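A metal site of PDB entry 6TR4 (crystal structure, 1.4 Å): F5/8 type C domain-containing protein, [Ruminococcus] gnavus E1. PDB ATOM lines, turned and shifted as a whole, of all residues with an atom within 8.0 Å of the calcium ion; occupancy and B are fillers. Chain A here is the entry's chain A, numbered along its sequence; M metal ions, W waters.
Within 4 Å of the calcium ion: Leu 188, Gly 197 and Glu 230.
The calcium ion is bound by O of Leu 188 (2.2 Å), O of Gly 197 (2.2 Å), OE2 of Glu 230 (2.3 Å), water W3 (2.3 Å), water W1 (2.4 Å), water W2 (2.4 Å) and water W4 (2.7 Å).
Water W1 lies within hydrogen-bond range of the side-chain hydroxyl of Tyr 236 (2.9 Å), the backbone carbonyl oxygen of Asn 229 (3.1 Å) and the side-chain carboxylate of Glu 230 (3.2 Å).
A ring nitrogen (ND1) of His 198 is in hydrogen-bond range of the side-chain carboxylate (OE1) of Glu 230 (2.7 Å).
OE1 of Glu 230 lies within hydrogen-bond range of N of Phe 199, 3.0 Å away.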
ATOM      1  N   LEU A 184     -13.207  -5.371  -9.068  1.00  0.00           N
ATOM      2  CA  LEU A 184     -13.333  -6.850  -9.134  1.00  0.00           C
ATOM      3  C   LEU A 184     -14.805  -7.215  -9.290  1.00  0.00           C
ATOM      4  O   LEU A 184     -15.154  -8.058 -10.135  1.00  0.00           O
ATOM      5  CB  LEU A 184     -12.789  -7.522  -7.861  1.00  0.00           C
ATOM      6  CG  LEU A 184     -11.279  -7.657  -7.744  1.00  0.00           C
ATOM      7  CD1 LEU A 184     -10.930  -8.172  -6.361  1.00  0.00           C
ATOM      8  CD2 LEU A 184     -10.714  -8.576  -8.797  1.00  0.00           C
ATOM      9  N   GLU A 185     -15.674  -6.656  -8.476  1.00  0.00           N
ATOM     10  CA  GLU A 185     -17.113  -6.986  -8.551  1.00  0.00           C
ATOM     11  C   GLU A 185     -17.669  -6.561  -9.899  1.00  0.00           C
ATOM     12  O   GLU A 185     -18.485  -7.294 -10.510  1.00  0.00           O
ATOM     13  CB  GLU A 185     -17.857  -6.328  -7.400  1.00  0.00           C
ATOM     14  CG  GLU A 185     -19.345  -6.588  -7.396  1.00  0.00           C
ATOM     15  CD  GLU A 185     -19.795  -8.025  -7.293  1.00  0.00           C
ATOM     16  OE1 GLU A 185     -19.065  -8.831  -6.635  1.00  0.00           O
ATOM     17  OE2 GLU A 185     -20.892  -8.322  -7.835  1.00  0.00           O
ATOM     18  N   GLU A 186     -17.272  -5.403 -10.379  1.00  0.00           N
ATOM     19  CA  GLU A 186     -17.814  -4.863 -11.641  1.00  0.00           C
ATOM     20  C   GLU A 186     -17.495  -5.811 -12.795  1.00  0.00           C
ATOM     21  O   GLU A 186     -18.380  -6.026 -13.644  1.00  0.00           O
ATOM     22  CB  GLU A 186     -17.219  -3.490 -11.920  1.00  0.00           C
ATOM     23  CG  GLU A 186     -17.767  -2.804 -13.135  1.00  0.00           C
ATOM     24  CD  GLU A 186     -17.232  -1.408 -13.316  1.00  0.00           C
ATOM     25  OE1 GLU A 186     -16.005  -1.238 -13.222  1.00  0.00           O
ATOM     26  OE2 GLU A 186     -18.079  -0.480 -13.521  1.00  0.00           O
ATOM     27  N   ILE A 187     -16.281  -6.320 -12.857  1.00  0.00           N
ATOM     28  CA  ILE A 187     -15.885  -7.247 -13.943  1.00  0.00           C
ATOM     29  C   ILE A 187     -16.472  -8.628 -13.672  1.00  0.00           C
ATOM     30  O   ILE A 187     -17.137  -9.206 -14.554  1.00  0.00           O
ATOM     31  CB  ILE A 187     -14.366  -7.296 -14.080  1.00  0.00           C
ATOM     32  CG1 ILE A 187     -13.797  -5.922 -14.464  1.00  0.00           C
ATOM     33  CG2 ILE A 187     -13.958  -8.378 -15.074  1.00  0.00           C
ATOM     34  CD1 ILE A 187     -12.304  -5.831 -14.370  1.00  0.00           C
ATOM     35  N   LEU A 188     -16.145  -9.216 -12.521  1.00  0.00           N
ATOM     36  CA  LEU A 188     -16.482 -10.632 -12.286  1.00  0.00           C
ATOM     37  C   LEU A 188     -17.996 -10.807 -12.189  1.00  0.00           C
ATOM     38  O   LEU A 188     -18.473 -11.915 -12.577  1.00  0.00           O
ATOM     39  CB  LEU A 188     -15.752 -11.124 -11.031  1.00  0.00           C
ATOM     40  CG  LEU A 188     -14.238 -11.059 -11.115  1.00  0.00           C
ATOM     41  CD1 LEU A 188     -13.648 -11.606  -9.818  1.00  0.00           C
ATOM     42  CD2 LEU A 188     -13.691 -11.830 -12.310  1.00  0.00           C
ATOM     43  N   GLY A 189     -18.732  -9.804 -11.703  1.00  0.00           N
ATOM     44  CA  GLY A 189     -20.185  -9.914 -11.572  1.00  0.00           C
ATOM     45  C   GLY A 189     -20.925  -9.677 -12.880  1.00  0.00           C
ATOM     46  O   GLY A 189     -22.150  -9.861 -12.861  1.00  0.00           O
ATOM     47  N   ASN A 190     -20.260  -9.295 -13.960  1.00  0.00           N
ATOM     48  CA  ASN A 190     -20.925  -8.987 -15.261  1.00  0.00           C
ATOM     49  C   ASN A 190     -20.639 -10.116 -16.225  1.00  0.00           C
ATOM     50  O   ASN A 190     -19.483 -10.351 -16.576  1.00  0.00           O
ATOM     51  CB  ASN A 190     -20.456  -7.643 -15.829  1.00  0.00           C
ATOM     52  CG  ASN A 190     -21.276  -7.178 -17.000  1.00  0.00           C
ATOM     53  OD1 ASN A 190     -21.741  -7.996 -17.786  1.00  0.00           O
ATOM     54  ND2 ASN A 190     -21.468  -5.859 -17.096  1.00  0.00           N
ATOM     55  N   PRO A 191     -21.654 -10.840 -16.734  1.00  0.00           N
ATOM     56  CA  PRO A 191     -21.411 -11.973 -17.606  1.00  0.00           C
ATOM     57  C   PRO A 191     -20.808 -11.632 -18.966  1.00  0.00           C
ATOM     58  O   PRO A 191     -20.362 -12.537 -19.656  1.00  0.00           O
ATOM     59  CB  PRO A 191     -22.796 -12.631 -17.771  1.00  0.00           C
ATOM     60  CG  PRO A 191     -23.785 -11.579 -17.340  1.00  0.00           C
ATOM     61  CD  PRO A 191     -23.073 -10.649 -16.403  1.00  0.00           C
ATOM     62  N   LYS A 192     -20.734 -10.368 -19.334  1.00  0.00           N
ATOM     63  CA  LYS A 192     -20.080  -9.995 -20.616  1.00  0.00           C
ATOM     64  C   LYS A 192     -18.562 -10.137 -20.506  1.00  0.00           C
ATOM     65  O   LYS A 192     -17.905 -10.102 -21.540  1.00  0.00           O
ATOM     66  CB  LYS A 192     -20.530  -8.608 -21.065  1.00  0.00           C
ATOM     67  CG  LYS A 192     -19.813  -7.441 -20.447  1.00  0.00           C
ATOM     68  CD  LYS A 192     -20.563  -6.158 -20.741  1.00  0.00           C
ATOM     69  CE  LYS A 192     -19.716  -4.953 -21.045  1.00  0.00           C
ATOM     70  NZ  LYS A 192     -20.597  -3.888 -21.586  1.00  0.00           N
ATOM     71  N   TYR A 193     -18.002 -10.384 -19.318  1.00  0.00           N
ATOM     72  CA  TYR A 193     -16.549 -10.599 -19.165  1.00  0.00           C
ATOM     73  C   TYR A 193     -16.272 -12.055 -18.775  1.00  0.00           C
ATOM     74  O   TYR A 193     -17.028 -12.639 -17.975  1.00  0.00           O
ATOM     75  CB  TYR A 193     -15.973  -9.660 -18.103  1.00  0.00           C
ATOM     76  CG  TYR A 193     -16.302  -8.206 -18.327  1.00  0.00           C
ATOM     77  CD1 TYR A 193     -15.865  -7.515 -19.458  1.00  0.00           C
ATOM     78  CD2 TYR A 193     -17.035  -7.481 -17.398  1.00  0.00           C
ATOM     79  CE1 TYR A 193     -16.158  -6.186 -19.651  1.00  0.00           C
ATOM     80  CE2 TYR A 193     -17.359  -6.157 -17.598  1.00  0.00           C
ATOM     81  CZ  TYR A 193     -16.914  -5.494 -18.718  1.00  0.00           C
ATOM     82  OH  TYR A 193     -17.224  -4.172 -18.877  1.00  0.00           O
ATOM     83  N   GLY A 194     -15.211 -12.611 -19.338  1.00  0.00           N
ATOM     84  CA  GLY A 194     -14.796 -13.999 -19.103  1.00  0.00           C
ATOM     85  C   GLY A 194     -15.208 -14.908 -20.245  1.00  0.00           C
ATOM     86  O   GLY A 194     -15.853 -14.452 -21.210  1.00  0.00           O
ATOM     87  N   ASN A 195     -14.886 -16.171 -20.115  1.00  0.00           N
ATOM     88  CA  ASN A 195     -15.410 -17.218 -21.021  1.00  0.00           C
ATOM     89  C   ASN A 195     -16.810 -17.587 -20.521  1.00  0.00           C
ATOM     90  O   ASN A 195     -16.891 -18.230 -19.481  1.00  0.00           O
ATOM     91  CB  ASN A 195     -14.482 -18.415 -21.041  1.00  0.00           C
ATOM     92  CG  ASN A 195     -14.972 -19.544 -21.910  1.00  0.00           C
ATOM     93  OD1 ASN A 195     -15.947 -19.369 -22.643  1.00  0.00           O
ATOM     94  ND2 ASN A 195     -14.334 -20.685 -21.809  1.00  0.00           N
ATOM     95  N   ASP A 196     -17.843 -17.170 -21.228  1.00  0.00           N
ATOM     96  CA  ASP A 196     -19.249 -17.391 -20.808  1.00  0.00           C
ATOM     97  C   ASP A 196     -19.395 -16.894 -19.372  1.00  0.00           C
ATOM     98  O   ASP A 196     -20.003 -17.594 -18.562  1.00  0.00           O
ATOM     99  CB  ASP A 196     -19.642 -18.866 -20.991  1.00  0.00           C
ATOM    100  CG  ASP A 196     -21.137 -19.133 -21.175  1.00  0.00           C
ATOM    101  OD1 ASP A 196     -21.939 -18.187 -21.158  1.00  0.00           O
ATOM    102  OD2 ASP A 196     -21.486 -20.311 -21.418  1.00  0.00           O
ATOM    103  N   GLY A 197     -18.842 -15.721 -19.057  1.00  0.00           N
ATOM    104  CA  GLY A 197     -19.010 -15.098 -17.736  1.00  0.00           C
ATOM    105  C   GLY A 197     -17.976 -15.546 -16.713  1.00  0.00           C
ATOM    106  O   GLY A 197     -17.970 -14.964 -15.593  1.00  0.00           O
ATOM    107  N   HIS A 198     -17.068 -16.454 -17.079  1.00  0.00           N
ATOM    108  CA  HIS A 198     -16.205 -17.100 -16.068  1.00  0.00           C
ATOM    109  C   HIS A 198     -14.727 -16.783 -16.273  1.00  0.00           C
ATOM    110  O   HIS A 198     -14.224 -16.821 -17.413  1.00  0.00           O
ATOM    111  CB  HIS A 198     -16.426 -18.613 -16.099  1.00  0.00           C
ATOM    112  CG  HIS A 198     -15.720 -19.389 -15.036  1.00  0.00           C
ATOM    113  ND1 HIS A 198     -15.690 -19.003 -13.700  1.00  0.00           N
ATOM    114  CD2 HIS A 198     -15.041 -20.546 -15.110  1.00  0.00           C
ATOM    115  CE1 HIS A 198     -15.043 -19.927 -13.015  1.00  0.00           C
ATOM    116  NE2 HIS A 198     -14.649 -20.903 -13.848  1.00  0.00           N
ATOM    117  N   PHE A 199     -14.021 -16.504 -15.174  1.00  0.00           N
ATOM    118  CA  PHE A 199     -12.544 -16.447 -15.130  1.00  0.00           C
ATOM    119  C   PHE A 199     -12.042 -17.572 -14.226  1.00  0.00           C
ATOM    120  O   PHE A 199     -12.648 -17.828 -13.184  1.00  0.00           O
ATOM    121  CB  PHE A 199     -12.085 -15.111 -14.559  1.00  0.00           C
ATOM    122  CG  PHE A 199     -12.318 -13.942 -15.473  1.00  0.00           C
ATOM    123  CD1 PHE A 199     -13.518 -13.250 -15.450  1.00  0.00           C
ATOM    124  CD2 PHE A 199     -11.338 -13.556 -16.374  1.00  0.00           C
ATOM    125  CE1 PHE A 199     -13.698 -12.148 -16.267  1.00  0.00           C
ATOM    126  CE2 PHE A 199     -11.529 -12.461 -17.210  1.00  0.00           C
ATOM    127  CZ  PHE A 199     -12.695 -11.760 -17.144  1.00  0.00           C
ATOM    128  N   ILE A 226     -13.837 -12.443  -5.330  1.00  0.00           N
ATOM    129  CA  ILE A 226     -13.429 -13.333  -6.449  1.00  0.00           C
ATOM    130  C   ILE A 226     -14.189 -14.643  -6.337  1.00  0.00           C
ATOM    131  O   ILE A 226     -14.770 -15.089  -7.344  1.00  0.00           O
ATOM    132  CB  ILE A 226     -11.909 -13.506  -6.459  1.00  0.00           C
ATOM    133  CG1 ILE A 226     -11.229 -12.190  -6.864  1.00  0.00           C
ATOM    134  CG2 ILE A 226     -11.530 -14.654  -7.389  1.00  0.00           C
ATOM    135  CD1 ILE A 226      -9.764 -12.127  -6.516  1.00  0.00           C
ATOM    136  N   ASP A 228     -16.882 -15.515  -4.585  1.00  0.00           N
ATOM    137  CA  ASP A 228     -18.364 -15.351  -4.647  1.00  0.00           C
ATOM    138  C   ASP A 228     -18.822 -15.221  -6.102  1.00  0.00           C
ATOM    139  O   ASP A 228     -20.005 -15.484  -6.373  1.00  0.00           O
ATOM    140  CB  ASP A 228     -18.812 -14.145  -3.823  1.00  0.00           C
ATOM    141  CG  ASP A 228     -18.754 -14.360  -2.321  1.00  0.00           C
ATOM    142  OD1 ASP A 228     -18.450 -15.496  -1.879  1.00  0.00           O
ATOM    143  OD2 ASP A 228     -19.086 -13.395  -1.617  1.00  0.00           O
ATOM    144  N   ASN A 229     -17.939 -14.841  -7.032  1.00  0.00           N
ATOM    145  CA  ASN A 229     -18.272 -14.702  -8.465  1.00  0.00           C
ATOM    146  C   ASN A 229     -17.747 -15.882  -9.289  1.00  0.00           C
ATOM    147  O   ASN A 229     -18.418 -16.248 -10.284  1.00  0.00           O
ATOM    148  CB  ASN A 229     -17.677 -13.420  -9.035  1.00  0.00           C
ATOM    149  CG  ASN A 229     -18.529 -12.237  -8.668  1.00  0.00           C
ATOM    150  OD1 ASN A 229     -19.608 -12.079  -9.242  1.00  0.00           O
ATOM    151  ND2 ASN A 229     -18.116 -11.431  -7.706  1.00  0.00           N
ATOM    152  N   GLU A 230     -16.605 -16.462  -8.944  1.00  0.00           N
ATOM    153  CA  GLU A 230     -15.861 -17.350  -9.874  1.00  0.00           C
ATOM    154  C   GLU A 230     -15.385 -18.629  -9.208  1.00  0.00           C
ATOM    155  O   GLU A 230     -14.708 -19.397  -9.888  1.00  0.00           O
ATOM    156  CB  GLU A 230     -14.654 -16.637 -10.469  1.00  0.00           C
ATOM    157  CG  GLU A 230     -14.972 -15.287 -11.096  1.00  0.00           C
ATOM    158  CD  GLU A 230     -15.923 -15.348 -12.284  1.00  0.00           C
ATOM    159  OE1 GLU A 230     -16.017 -16.408 -12.931  1.00  0.00           O
ATOM    160  OE2 GLU A 230     -16.590 -14.313 -12.557  1.00  0.00           O
ATOM    161  N   ALA A 234     -19.788 -19.656  -5.968  1.00  0.00           N
ATOM    162  CA  ALA A 234     -20.569 -19.276  -7.168  1.00  0.00           C
ATOM    163  C   ALA A 234     -21.075 -20.525  -7.907  1.00  0.00           C
ATOM    164  O   ALA A 234     -21.666 -20.365  -8.991  1.00  0.00           O
ATOM    165  CB  ALA A 234     -19.718 -18.405  -8.059  1.00  0.00           C
ATOM    166  N   TYR A 236     -19.102 -23.170  -9.078  1.00  0.00           N
ATOM    167  CA  TYR A 236     -18.055 -23.832  -9.898  1.00  0.00           C
ATOM    168  C   TYR A 236     -17.431 -24.981  -9.084  1.00  0.00           C
ATOM    169  O   TYR A 236     -17.579 -25.050  -7.857  1.00  0.00           O
ATOM    170  CB  TYR A 236     -17.025 -22.817 -10.370  1.00  0.00           C
ATOM    171  CG  TYR A 236     -17.593 -21.771 -11.288  1.00  0.00           C
ATOM    172  CD1 TYR A 236     -17.783 -22.036 -12.639  1.00  0.00           C
ATOM    173  CD2 TYR A 236     -17.975 -20.525 -10.811  1.00  0.00           C
ATOM    174  CE1 TYR A 236     -18.346 -21.105 -13.485  1.00  0.00           C
ATOM    175  CE2 TYR A 236     -18.524 -19.563 -11.643  1.00  0.00           C
ATOM    176  CZ  TYR A 236     -18.705 -19.857 -12.984  1.00  0.00           C
ATOM    177  OH  TYR A 236     -19.217 -18.910 -13.822  1.00  0.00           O
HETATM  178 CA    CA M   1     -18.446 -13.817 -13.741  1.00  0.00          CA
HETATM  179  O   HOH W   1     -19.180 -16.072 -13.264  1.00  0.00           O
HETATM  180  O   HOH W   2     -17.435 -12.162 -15.237  1.00  0.00           O
HETATM  181  O   HOH W   3     -20.604 -13.580 -14.593  1.00  0.00           O
HETATM  182  O   HOH W   4     -19.899 -13.950 -11.438  1.00  0.00           O
